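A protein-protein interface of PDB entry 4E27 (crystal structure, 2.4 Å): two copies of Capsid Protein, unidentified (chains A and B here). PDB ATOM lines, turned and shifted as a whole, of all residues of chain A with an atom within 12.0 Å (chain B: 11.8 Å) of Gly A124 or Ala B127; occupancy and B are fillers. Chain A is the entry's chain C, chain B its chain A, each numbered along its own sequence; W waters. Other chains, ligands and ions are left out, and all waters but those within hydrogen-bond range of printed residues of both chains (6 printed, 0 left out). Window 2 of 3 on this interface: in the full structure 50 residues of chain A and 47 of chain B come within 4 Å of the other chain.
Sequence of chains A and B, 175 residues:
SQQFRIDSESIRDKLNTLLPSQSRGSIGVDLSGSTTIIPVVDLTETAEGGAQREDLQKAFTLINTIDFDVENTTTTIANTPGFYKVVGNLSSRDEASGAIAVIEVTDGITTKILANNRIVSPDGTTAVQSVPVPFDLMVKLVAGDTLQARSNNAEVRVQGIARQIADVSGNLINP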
ATOM      1  N   ASP A  94     -17.359  27.277 -33.795  1.00  0.00           N
ATOM      2  CA  ASP A  94     -17.249  27.165 -32.350  1.00  0.00           C
ATOM      3  C   ASP A  94     -15.876  27.666 -31.922  1.00  0.00           C
ATOM      4  O   ASP A  94     -14.893  27.517 -32.649  1.00  0.00           O
ATOM      5  CB  ASP A  94     -17.407  25.685 -31.967  1.00  0.00           C
ATOM      6  CG  ASP A  94     -17.585  25.465 -30.467  1.00  0.00           C
ATOM      7  OD1 ASP A  94     -16.749  25.938 -29.661  1.00  0.00           O
ATOM      8  OD2 ASP A  94     -18.568  24.793 -30.096  1.00  0.00           O
ATOM      9  N   GLU A  95     -15.792  28.244 -30.736  1.00  0.00           N
ATOM     10  CA  GLU A  95     -14.515  28.756 -30.263  1.00  0.00           C
ATOM     11  C   GLU A  95     -13.497  27.636 -30.018  1.00  0.00           C
ATOM     12  O   GLU A  95     -12.299  27.889 -29.984  1.00  0.00           O
ATOM     13  CB  GLU A  95     -14.702  29.631 -29.016  1.00  0.00           C
ATOM     14  CG  GLU A  95     -15.416  28.950 -27.839  1.00  0.00           C
ATOM     15  CD  GLU A  95     -14.484  28.102 -26.988  1.00  0.00           C
ATOM     16  OE1 GLU A  95     -14.945  27.071 -26.446  1.00  0.00           O
ATOM     17  OE2 GLU A  95     -13.294  28.466 -26.865  1.00  0.00           O
ATOM     18  N   VAL A 120     -18.097  31.513 -31.708  1.00  0.00           N
ATOM     19  CA  VAL A 120     -19.389  31.074 -31.170  1.00  0.00           C
ATOM     20  C   VAL A 120     -19.266  30.029 -30.054  1.00  0.00           C
ATOM     21  O   VAL A 120     -18.318  29.244 -30.002  1.00  0.00           O
ATOM     22  CB  VAL A 120     -20.426  30.662 -32.256  1.00  0.00           C
ATOM     23  CG1 VAL A 120     -20.331  31.579 -33.486  1.00  0.00           C
ATOM     24  CG2 VAL A 120     -20.278  29.210 -32.642  1.00  0.00           C
ATOM     25  N   SER A 121     -20.235  30.055 -29.149  1.00  0.00           N
ATOM     26  CA  SER A 121     -20.229  29.199 -27.978  1.00  0.00           C
ATOM     27  C   SER A 121     -21.631  28.631 -27.793  1.00  0.00           C
ATOM     28  O   SER A 121     -22.408  29.131 -26.982  1.00  0.00           O
ATOM     29  CB  SER A 121     -19.827  30.025 -26.756  1.00  0.00           C
ATOM     30  OG  SER A 121     -19.798  29.245 -25.584  1.00  0.00           O
ATOM     31  N   PRO A 122     -21.971  27.592 -28.573  1.00  0.00           N
ATOM     32  CA  PRO A 122     -23.303  26.987 -28.480  1.00  0.00           C
ATOM     33  C   PRO A 122     -23.433  26.177 -27.193  1.00  0.00           C
ATOM     34  O   PRO A 122     -22.443  25.658 -26.676  1.00  0.00           O
ATOM     35  CB  PRO A 122     -23.336  26.057 -29.684  1.00  0.00           C
ATOM     36  CG  PRO A 122     -21.892  25.665 -29.869  1.00  0.00           C
ATOM     37  CD  PRO A 122     -21.091  26.869 -29.505  1.00  0.00           C
ATOM     38  N   ASP A 123     -24.651  26.082 -26.676  1.00  0.00           N
ATOM     39  CA  ASP A 123     -24.890  25.358 -25.442  1.00  0.00           C
ATOM     40  C   ASP A 123     -26.047  24.384 -25.599  1.00  0.00           C
ATOM     41  O   ASP A 123     -27.107  24.754 -26.093  1.00  0.00           O
ATOM     42  CB  ASP A 123     -25.202  26.339 -24.323  1.00  0.00           C
ATOM     43  CG  ASP A 123     -25.258  25.669 -22.982  1.00  0.00           C
ATOM     44  OD1 ASP A 123     -24.316  24.903 -22.682  1.00  0.00           O
ATOM     45  OD2 ASP A 123     -26.248  25.889 -22.241  1.00  0.00           O
ATOM     46  N   GLY A 124     -25.845  23.138 -25.181  1.00  0.00           N
ATOM     47  CA  GLY A 124     -26.926  22.164 -25.159  1.00  0.00           C
ATOM     48  C   GLY A 124     -27.158  21.551 -26.530  1.00  0.00           C
ATOM     49  O   GLY A 124     -28.238  20.986 -26.786  1.00  0.00           O
ATOM     50  N   THR A 125     -26.148  21.664 -27.405  1.00  0.00           N
ATOM     51  CA  THR A 125     -26.211  21.072 -28.739  1.00  0.00           C
ATOM     52  C   THR A 125     -24.835  20.938 -29.395  1.00  0.00           C
ATOM     53  O   THR A 125     -23.911  21.652 -29.050  1.00  0.00           O
ATOM     54  CB  THR A 125     -27.133  21.889 -29.674  1.00  0.00           C
ATOM     55  OG1 THR A 125     -27.071  21.356 -31.002  1.00  0.00           O
ATOM     56  CG2 THR A 125     -26.703  23.325 -29.719  1.00  0.00           C
ATOM     57  N   THR A 126     -24.713  20.016 -30.345  1.00  0.00           N
ATOM     58  CA  THR A 126     -23.509  19.898 -31.155  1.00  0.00           C
ATOM     59  C   THR A 126     -23.862  20.219 -32.608  1.00  0.00           C
ATOM     60  O   THR A 126     -23.021  20.126 -33.509  1.00  0.00           O
ATOM     61  CB  THR A 126     -22.906  18.492 -31.071  1.00  0.00           C
ATOM     62  OG1 THR A 126     -23.836  17.551 -31.617  1.00  0.00           O
ATOM     63  CG2 THR A 126     -22.596  18.117 -29.601  1.00  0.00           C
ATOM     64  N   ALA A 127     -25.115  20.589 -32.831  1.00  0.00           N
ATOM     65  CA  ALA A 127     -25.535  21.062 -34.146  1.00  0.00           C
ATOM     66  C   ALA A 127     -25.308  22.566 -34.189  1.00  0.00           C
ATOM     67  O   ALA A 127     -26.195  23.341 -33.841  1.00  0.00           O
ATOM     68  CB  ALA A 127     -27.003  20.726 -34.400  1.00  0.00           C
ATOM     69  N   VAL A 128     -24.110  22.964 -34.613  1.00  0.00           N
ATOM     70  CA  VAL A 128     -23.632  24.336 -34.467  1.00  0.00           C
ATOM     71  C   VAL A 128     -23.830  25.179 -35.722  1.00  0.00           C
ATOM     72  O   VAL A 128     -23.080  25.043 -36.695  1.00  0.00           O
ATOM     73  CB  VAL A 128     -22.135  24.351 -34.086  1.00  0.00           C
ATOM     74  CG1 VAL A 128     -21.580  25.776 -34.065  1.00  0.00           C
ATOM     75  CG2 VAL A 128     -21.923  23.657 -32.742  1.00  0.00           C
ATOM     76  N   GLN A 129     -24.844  26.044 -35.694  1.00  0.00           N
ATOM     77  CA  GLN A 129     -25.102  26.944 -36.808  1.00  0.00           C
ATOM     78  C   GLN A 129     -23.979  27.964 -36.904  1.00  0.00           C
ATOM     79  O   GLN A 129     -23.335  28.305 -35.901  1.00  0.00           O
ATOM     80  CB  GLN A 129     -26.451  27.655 -36.658  1.00  0.00           C
ATOM     81  CG  GLN A 129     -27.671  26.719 -36.540  1.00  0.00           C
ATOM     82  CD  GLN A 129     -27.974  25.954 -37.819  1.00  0.00           C
ATOM     83  OE1 GLN A 129     -27.627  26.392 -38.917  1.00  0.00           O
ATOM     84  NE2 GLN A 129     -28.642  24.814 -37.681  1.00  0.00           N
ATOM     85  N   SER A 130     -23.756  28.448 -38.122  1.00  0.00           N
ATOM     86  CA  SER A 130     -22.662  29.360 -38.417  1.00  0.00           C
ATOM     87  C   SER A 130     -23.187  30.604 -39.128  1.00  0.00           C
ATOM     88  O   SER A 130     -24.139  30.538 -39.907  1.00  0.00           O
ATOM     89  CB  SER A 130     -21.623  28.633 -39.276  1.00  0.00           C
ATOM     90  OG  SER A 130     -20.600  29.493 -39.758  1.00  0.00           O
ATOM     91  N   SER B  92     -21.718  35.085 -27.739  1.00  0.00           N
ATOM     92  CA  SER B  92     -23.016  35.337 -27.134  1.00  0.00           C
ATOM     93  C   SER B  92     -23.428  34.106 -26.349  1.00  0.00           C
ATOM     94  O   SER B  92     -23.185  32.974 -26.774  1.00  0.00           O
ATOM     95  CB  SER B  92     -24.074  35.648 -28.185  1.00  0.00           C
ATOM     96  OG  SER B  92     -24.516  34.460 -28.807  1.00  0.00           O
ATOM     97  N   ARG B  93     -24.044  34.331 -25.198  1.00  0.00           N
ATOM     98  CA  ARG B  93     -24.606  33.254 -24.416  1.00  0.00           C
ATOM     99  C   ARG B  93     -25.961  33.728 -23.956  1.00  0.00           C
ATOM    100  O   ARG B  93     -26.280  34.930 -24.063  1.00  0.00           O
ATOM    101  CB  ARG B  93     -23.737  32.931 -23.189  1.00  0.00           C
ATOM    102  CG  ARG B  93     -22.380  32.321 -23.498  1.00  0.00           C
ATOM    103  CD  ARG B  93     -22.495  30.930 -24.078  1.00  0.00           C
ATOM    104  NE  ARG B  93     -22.998  29.985 -23.089  1.00  0.00           N
ATOM    105  CZ  ARG B  93     -22.338  28.909 -22.665  1.00  0.00           C
ATOM    106  NH1 ARG B  93     -21.147  28.620 -23.163  1.00  0.00           N
ATOM    107  NH2 ARG B  93     -22.880  28.109 -21.754  1.00  0.00           N
ATOM    108  N   ASP B  94     -26.736  32.782 -23.431  1.00  0.00           N
ATOM    109  CA  ASP B  94     -28.039  33.057 -22.857  1.00  0.00           C
ATOM    110  C   ASP B  94     -27.876  34.117 -21.763  1.00  0.00           C
ATOM    111  O   ASP B  94     -26.881  34.129 -21.052  1.00  0.00           O
ATOM    112  CB  ASP B  94     -28.635  31.750 -22.279  1.00  0.00           C
ATOM    113  CG  ASP B  94     -30.111  31.880 -21.891  1.00  0.00           C
ATOM    114  OD1 ASP B  94     -30.466  32.798 -21.107  1.00  0.00           O
ATOM    115  OD2 ASP B  94     -30.920  31.053 -22.374  1.00  0.00           O
ATOM    116  N   GLU B  95     -28.859  35.000 -21.633  1.00  0.00           N
ATOM    117  CA  GLU B  95     -28.834  36.008 -20.592  1.00  0.00           C
ATOM    118  C   GLU B  95     -28.841  35.361 -19.200  1.00  0.00           C
ATOM    119  O   GLU B  95     -28.456  35.995 -18.220  1.00  0.00           O
ATOM    120  CB  GLU B  95     -30.015  36.977 -20.749  1.00  0.00           C
ATOM    121  CG  GLU B  95     -31.396  36.345 -20.583  1.00  0.00           C
ATOM    122  CD  GLU B  95     -31.820  36.232 -19.126  1.00  0.00           C
ATOM    123  OE1 GLU B  95     -32.591  35.295 -18.784  1.00  0.00           O
ATOM    124  OE2 GLU B  95     -31.369  37.084 -18.322  1.00  0.00           O
ATOM    125  N   SER B  97     -27.135  32.616 -18.517  1.00  0.00           N
ATOM    126  CA  SER B  97     -25.909  31.831 -18.427  1.00  0.00           C
ATOM    127  C   SER B  97     -25.016  32.321 -17.309  1.00  0.00           C
ATOM    128  O   SER B  97     -25.122  33.465 -16.877  1.00  0.00           O
ATOM    129  CB  SER B  97     -25.129  31.891 -19.744  1.00  0.00           C
ATOM    130  OG  SER B  97     -23.950  31.096 -19.678  1.00  0.00           O
ATOM    131  N   ALA B  99     -21.810  31.947 -17.993  1.00  0.00           N
ATOM    132  CA  ALA B  99     -20.595  32.114 -18.804  1.00  0.00           C
ATOM    133  C   ALA B  99     -20.426  33.547 -19.307  1.00  0.00           C
ATOM    134  O   ALA B  99     -21.222  34.044 -20.122  1.00  0.00           O
ATOM    135  CB  ALA B  99     -20.578  31.121 -19.964  1.00  0.00           C
ATOM    136  N   VAL B 120     -28.751  36.802 -25.213  1.00  0.00           N
ATOM    137  CA  VAL B 120     -29.754  36.106 -26.011  1.00  0.00           C
ATOM    138  C   VAL B 120     -30.852  35.503 -25.125  1.00  0.00           C
ATOM    139  O   VAL B 120     -30.626  35.198 -23.951  1.00  0.00           O
ATOM    140  CB  VAL B 120     -29.147  35.056 -26.995  1.00  0.00           C
ATOM    141  CG1 VAL B 120     -27.856  35.567 -27.612  1.00  0.00           C
ATOM    142  CG2 VAL B 120     -28.918  33.719 -26.312  1.00  0.00           C
ATOM    143  N   SER B 121     -32.038  35.337 -25.708  1.00  0.00           N
ATOM    144  CA  SER B 121     -33.214  34.905 -24.976  1.00  0.00           C
ATOM    145  C   SER B 121     -33.994  33.883 -25.802  1.00  0.00           C
ATOM    146  O   SER B 121     -35.040  34.200 -26.365  1.00  0.00           O
ATOM    147  CB  SER B 121     -34.094  36.107 -24.671  1.00  0.00           C
ATOM    148  OG  SER B 121     -35.012  35.828 -23.636  1.00  0.00           O
ATOM    149  N   PRO B 122     -33.467  32.652 -25.892  1.00  0.00           N
ATOM    150  CA  PRO B 122     -34.102  31.586 -26.664  1.00  0.00           C
ATOM    151  C   PRO B 122     -35.412  31.169 -26.019  1.00  0.00           C
ATOM    152  O   PRO B 122     -35.585  31.362 -24.827  1.00  0.00           O
ATOM    153  CB  PRO B 122     -33.093  30.443 -26.559  1.00  0.00           C
ATOM    154  CG  PRO B 122     -32.383  30.702 -25.266  1.00  0.00           C
ATOM    155  CD  PRO B 122     -32.247  32.185 -25.208  1.00  0.00           C
ATOM    156  N   ASP B 123     -36.320  30.596 -26.795  1.00  0.00           N
ATOM    157  CA  ASP B 123     -37.610  30.210 -26.258  1.00  0.00           C
ATOM    158  C   ASP B 123     -38.054  28.869 -26.832  1.00  0.00           C
ATOM    159  O   ASP B 123     -37.989  28.657 -28.040  1.00  0.00           O
ATOM    160  CB  ASP B 123     -38.636  31.285 -26.576  1.00  0.00           C
ATOM    161  CG  ASP B 123     -39.953  31.043 -25.891  1.00  0.00           C
ATOM    162  OD1 ASP B 123     -39.954  30.799 -24.659  1.00  0.00           O
ATOM    163  OD2 ASP B 123     -40.980  31.085 -26.596  1.00  0.00           O
ATOM    164  N   GLY B 124     -38.506  27.966 -25.968  1.00  0.00           N
ATOM    165  CA  GLY B 124     -38.942  26.646 -26.417  1.00  0.00           C
ATOM    166  C   GLY B 124     -37.809  25.744 -26.882  1.00  0.00           C
ATOM    167  O   GLY B 124     -38.036  24.797 -27.636  1.00  0.00           O
ATOM    168  N   THR B 125     -36.585  26.036 -26.433  1.00  0.00           N
ATOM    169  CA  THR B 125     -35.446  25.136 -26.639  1.00  0.00           C
ATOM    170  C   THR B 125     -34.336  25.376 -25.621  1.00  0.00           C
ATOM    171  O   THR B 125     -34.233  26.461 -25.071  1.00  0.00           O
ATOM    172  CB  THR B 125     -34.857  25.276 -28.058  1.00  0.00           C
ATOM    173  OG1 THR B 125     -33.717  24.421 -28.188  1.00  0.00           O
ATOM    174  CG2 THR B 125     -34.431  26.705 -28.335  1.00  0.00           C
ATOM    175  N   THR B 126     -33.518  24.355 -25.366  1.00  0.00           N
ATOM    176  CA  THR B 126     -32.346  24.480 -24.510  1.00  0.00           C
ATOM    177  C   THR B 126     -31.084  24.269 -25.351  1.00  0.00           C
ATOM    178  O   THR B 126     -29.969  24.268 -24.837  1.00  0.00           O
ATOM    179  CB  THR B 126     -32.346  23.446 -23.378  1.00  0.00           C
ATOM    180  OG1 THR B 126     -32.130  22.146 -23.930  1.00  0.00           O
ATOM    181  CG2 THR B 126     -33.678  23.464 -22.611  1.00  0.00           C
ATOM    182  N   ALA B 127     -31.280  24.057 -26.643  1.00  0.00           N
ATOM    183  CA  ALA B 127     -30.183  24.006 -27.588  1.00  0.00           C
ATOM    184  C   ALA B 127     -30.018  25.432 -28.074  1.00  0.00           C
ATOM    185  O   ALA B 127     -30.759  25.887 -28.951  1.00  0.00           O
ATOM    186  CB  ALA B 127     -30.523  23.077 -28.747  1.00  0.00           C
ATOM    187  N   VAL B 128     -29.059  26.138 -27.480  1.00  0.00           N
ATOM    188  CA  VAL B 128     -28.965  27.585 -27.604  1.00  0.00           C
ATOM    189  C   VAL B 128     -27.831  27.992 -28.526  1.00  0.00           C
ATOM    190  O   VAL B 128     -26.655  27.962 -28.130  1.00  0.00           O
ATOM    191  CB  VAL B 128     -28.750  28.251 -26.220  1.00  0.00           C
ATOM    192  CG1 VAL B 128     -28.598  29.743 -26.371  1.00  0.00           C
ATOM    193  CG2 VAL B 128     -29.910  27.936 -25.288  1.00  0.00           C
ATOM    194  N   GLN B 129     -28.188  28.360 -29.757  1.00  0.00           N
ATOM    195  CA  GLN B 129     -27.214  28.818 -30.745  1.00  0.00           C
ATOM    196  C   GLN B 129     -26.559  30.114 -30.288  1.00  0.00           C
ATOM    197  O   GLN B 129     -27.176  30.929 -29.591  1.00  0.00           O
ATOM    198  CB  GLN B 129     -27.877  29.041 -32.111  1.00  0.00           C
ATOM    199  CG  GLN B 129     -28.507  27.791 -32.719  1.00  0.00           C
ATOM    200  CD  GLN B 129     -27.486  26.717 -33.032  1.00  0.00           C
ATOM    201  OE1 GLN B 129     -26.345  27.014 -33.409  1.00  0.00           O
ATOM    202  NE2 GLN B 129     -27.887  25.462 -32.880  1.00  0.00           N
ATOM    203  N   SER B 130     -25.316  30.305 -30.711  1.00  0.00           N
ATOM    204  CA  SER B 130     -24.532  31.462 -30.307  1.00  0.00           C
ATOM    205  C   SER B 130     -23.945  32.183 -31.516  1.00  0.00           C
ATOM    206  O   SER B 130     -23.576  31.544 -32.498  1.00  0.00           O
ATOM    207  CB  SER B 130     -23.407  31.016 -29.377  1.00  0.00           C
ATOM    208  OG  SER B 130     -22.525  32.081 -29.104  1.00  0.00           O
ATOM    209  N   VAL B 131     -23.853  33.509 -31.430  1.00  0.00           N
ATOM    210  CA  VAL B 131     -23.311  34.334 -32.512  1.00  0.00           C
ATOM    211  C   VAL B 131     -22.267  35.280 -31.929  1.00  0.00           C
ATOM    212  O   VAL B 131     -22.191  35.440 -30.709  1.00  0.00           O
ATOM    213  CB  VAL B 131     -24.417  35.179 -33.215  1.00  0.00           C
ATOM    214  CG1 VAL B 131     -25.385  34.294 -33.999  1.00  0.00           C
ATOM    215  CG2 VAL B 131     -25.163  36.069 -32.206  1.00  0.00           C
ATOM    216  N   ASN B 153     -14.898  31.591 -18.234  1.00  0.00           N
ATOM    217  CA  ASN B 153     -15.147  30.218 -18.631  1.00  0.00           C
ATOM    218  C   ASN B 153     -14.396  29.886 -19.907  1.00  0.00           C
ATOM    219  O   ASN B 153     -14.209  30.747 -20.751  1.00  0.00           O
ATOM    220  CB  ASN B 153     -16.646  30.009 -18.847  1.00  0.00           C
ATOM    221  CG  ASN B 153     -17.026  28.552 -18.853  1.00  0.00           C
ATOM    222  OD1 ASN B 153     -16.638  27.805 -19.746  1.00  0.00           O
ATOM    223  ND2 ASN B 153     -17.789  28.136 -17.855  1.00  0.00           N
ATOM    224  N   GLU B 155     -15.370  28.156 -22.325  1.00  0.00           N
ATOM    225  CA  GLU B 155     -16.285  28.000 -23.452  1.00  0.00           C
ATOM    226  C   GLU B 155     -16.613  29.322 -24.130  1.00  0.00           C
ATOM    227  O   GLU B 155     -17.220  29.332 -25.200  1.00  0.00           O
ATOM    228  CB  GLU B 155     -17.597  27.354 -23.006  1.00  0.00           C
ATOM    229  CG  GLU B 155     -17.529  25.869 -22.747  1.00  0.00           C
ATOM    230  CD  GLU B 155     -18.804  25.352 -22.128  1.00  0.00           C
ATOM    231  OE1 GLU B 155     -19.743  26.149 -21.912  1.00  0.00           O
ATOM    232  OE2 GLU B 155     -18.874  24.141 -21.856  1.00  0.00           O
ATOM    233  N   VAL B 156     -16.241  30.437 -23.506  1.00  0.00           N
ATOM    234  CA  VAL B 156     -16.553  31.745 -24.089  1.00  0.00           C
ATOM    235  C   VAL B 156     -15.325  32.636 -24.265  1.00  0.00           C
ATOM    236  O   VAL B 156     -14.409  32.640 -23.425  1.00  0.00           O
ATOM    237  CB  VAL B 156     -17.667  32.486 -23.314  1.00  0.00           C
ATOM    238  CG1 VAL B 156     -18.955  31.690 -23.365  1.00  0.00           C
ATOM    239  CG2 VAL B 156     -17.240  32.757 -21.861  1.00  0.00           C
HETATM  240  O   HOH W   1     -28.824  24.970 -22.608  1.00  0.00           O
HETATM  241  O   HOH W   2     -21.793  24.564 -23.347  1.00  0.00           O
HETATM  242  O   HOH W   3     -30.250  20.712 -25.131  1.00  0.00           O
HETATM  243  O   HOH W   4     -25.198  28.577 -20.400  1.00  0.00           O
HETATM  244  O   HOH W   5     -25.151  29.684 -26.574  1.00  0.00           O
HETATM  245  O   HOH W   6     -24.348  31.223 -35.531  1.00  0.00           O
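Val A120 touches Ser B130.
Ser A121 touches Ser B92 (O to O, 3.9 Å).
Pro A122 touches Val B128 (CA to O, 3.5 Å).
Pro A122 touches Ser B130 (N to CB, 3.8 Å).
O of Asp A123 touches CA of Ala B127 (3.5 Å).
CA of Gly A124 touches O of Thr B126, 3.7 Å away.
CB of Ala B127 touches O of Gly A124 (3.7 Å).
Ala B127 touches Thr A125 (CB to CB, 3.7 Å).
Gln B129 touches Thr A125 (NE2 to CG2, 3.995 Å).
C of Val A128 touches OE1 of Gln B129, at 3.9 Å.
Val A120 touches Ser B130, but with the chains exchanged Ser A130 does not touch Val B120 (13.3 Å).
Gly A124 touches Ala B127, but with the chains exchanged Ala A127 does not touch Gly B124 (13.4 Å).
Thr A125 touches Ala B127, but with the chains exchanged Ala A127 does not touch Thr B125 (9.5 Å).
Val A128 touches Gln B129, but with the chains exchanged Gln A129 does not touch Val B128 (8.0 Å).
13 positions are printed for both chains.
Of the 20 pairs that touch across the chains among the printed residues, 1 has its exchanged pair printed and touching as well.
N of Ala A127 sits at hydrogen-bond distance from OG1 of Thr A125 (2.8 Å).
The side-chain amide oxygen (OD1) of Asn B153 sits at hydrogen-bond distance from the backbone NH (N) of Glu B155.
The backbone carbonyl oxygen (O) of Arg B93 is in hydrogen-bond range of the backbone NH (N) of Val B120 (3.3 Å).
OG1 of Thr B125 is in hydrogen-bond range of N of Ala B127 (2.9 Å).
The backbone carbonyl oxygen (O) of Ser B92 lies within hydrogen-bond range of the side-chain hydroxyl (OG) of Ser B130, at 2.6 Å.
O of Val A120 lies within hydrogen-bond range of N of Glu A95 (2.8 Å).
Hydrophobic or aromatic side chains of chain A within 4 Å of the printed part of chain B: Val A120.
Of the 21 printed residues of chain B, 9 touch a printed residue of chain A.
Hydrophobic or aromatic side chains of chain B within 4 Å of the printed part of chain A: Ala B127, Val B128 and Val B156.
Among the printed residues, Asp or Glu carboxylates within 4 Å of a Lys or Arg side-chain nitrogen of the other chain: Asp A123 with Arg B93 (3.6 Å).
The backbone NH (N) of Ser A121 is in hydrogen-bond range of the side-chain hydroxyl (OG) of Ser B130 (3.1 Å).
The backbone NH (N) of Val B128 sits at hydrogen-bond distance from the backbone carbonyl oxygen (O) of Asp A123.
The backbone carbonyl oxygen (O) of Glu B155 is in hydrogen-bond range of the side-chain hydroxyl (OG) of Ser A121.
The side-chain amide nitrogen of Gln B129 sits at hydrogen-bond distance from the backbone carbonyl oxygen of Ala A127.
The backbone carbonyl oxygen (O) of Asp A123 sits close to the backbone carbonyl oxygen (O) of Thr B126 (3.2 Å).
OE1 of Gln B129 sits at hydrogen-bond distance from N of Gln A129 (2.9 Å).
O of Glu B155 sits close to OE1 of Glu A95 (3.4 Å).
The guanidinium group (NH2) of Arg B93 lies within salt-bridge range of the side-chain carboxylate (OD1) of Asp A123 (3.6 Å).
NH1 of Arg B93 sits at hydrogen-bond distance from OG of Ser A121 (2.8 Å).
Water W1 lies within hydrogen-bond range of the backbone carbonyl oxygen (O) of Thr B126 (2.6 Å) and the side-chain carboxylate (OD2) of Asp A123 (2.8 Å).
Water W3 lies within hydrogen-bond range of O of Gly A124 (2.6 Å) and OG1 of Thr B126 (2.7 Å).
Water W2 lies within hydrogen-bond range of OD1 of Asp A123 and OE1 of Glu B155.
Water W4 lies within hydrogen-bond range of the guanidinium group (NH2) of Arg B93 (2.7 Å), the side-chain hydroxyl (OG) of Ser B97 (2.9 Å) and the side-chain carboxylate (OD2) of Asp A123 (3.4 Å).
Water W5 bridges O of Val B128 and O of Ser A121.
Water W6 bridges the backbone carbonyl oxygen (O) of Gln A129 (3.1 Å) and the backbone carbonyl oxygen (O) of Ser B130 (3.1 Å).
Printed residues of chain B within 4 Å of Val A120: Ser B130 (3.3 Å).
Of chain B, only Val B128 and Ser B130 come within 4 Å of Pro A122.
Of chain B, only Arg B93, Thr B126, Ala B127 and Val B128 come within 4 Å of Asp A123.
Gly A124 touches just these residues of chain B: Thr B126 (3.7 Å) and Ala B127 (3.7 Å).
Gly B124 touches none of the printed residues of chain A.
No residue of chain A comes within 4 Å of Thr B125.
Of chain A, only Asp A123 and Gly A124 come within 4 Å of Thr B126.
Val B128 touches just these residues of chain A: Pro A122 and Asp A123.
Of the printed residues of chain A, Glu B155 touches Glu A95 (3.2 Å) and Ser A121 (2.6 Å).
Printed residues of chain A within 4 Å of Val B156: Ser A121.
The nearest residue of chain B that does not touch Gly A124 is Val B128 (5.0 Å).
The nearest printed residue of chain A that does not touch Ala B127 is Pro A122 (6.7 Å).
The nearest printed residue of chain B that does not touch Glu A95 is Val B156 (4.5 Å).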
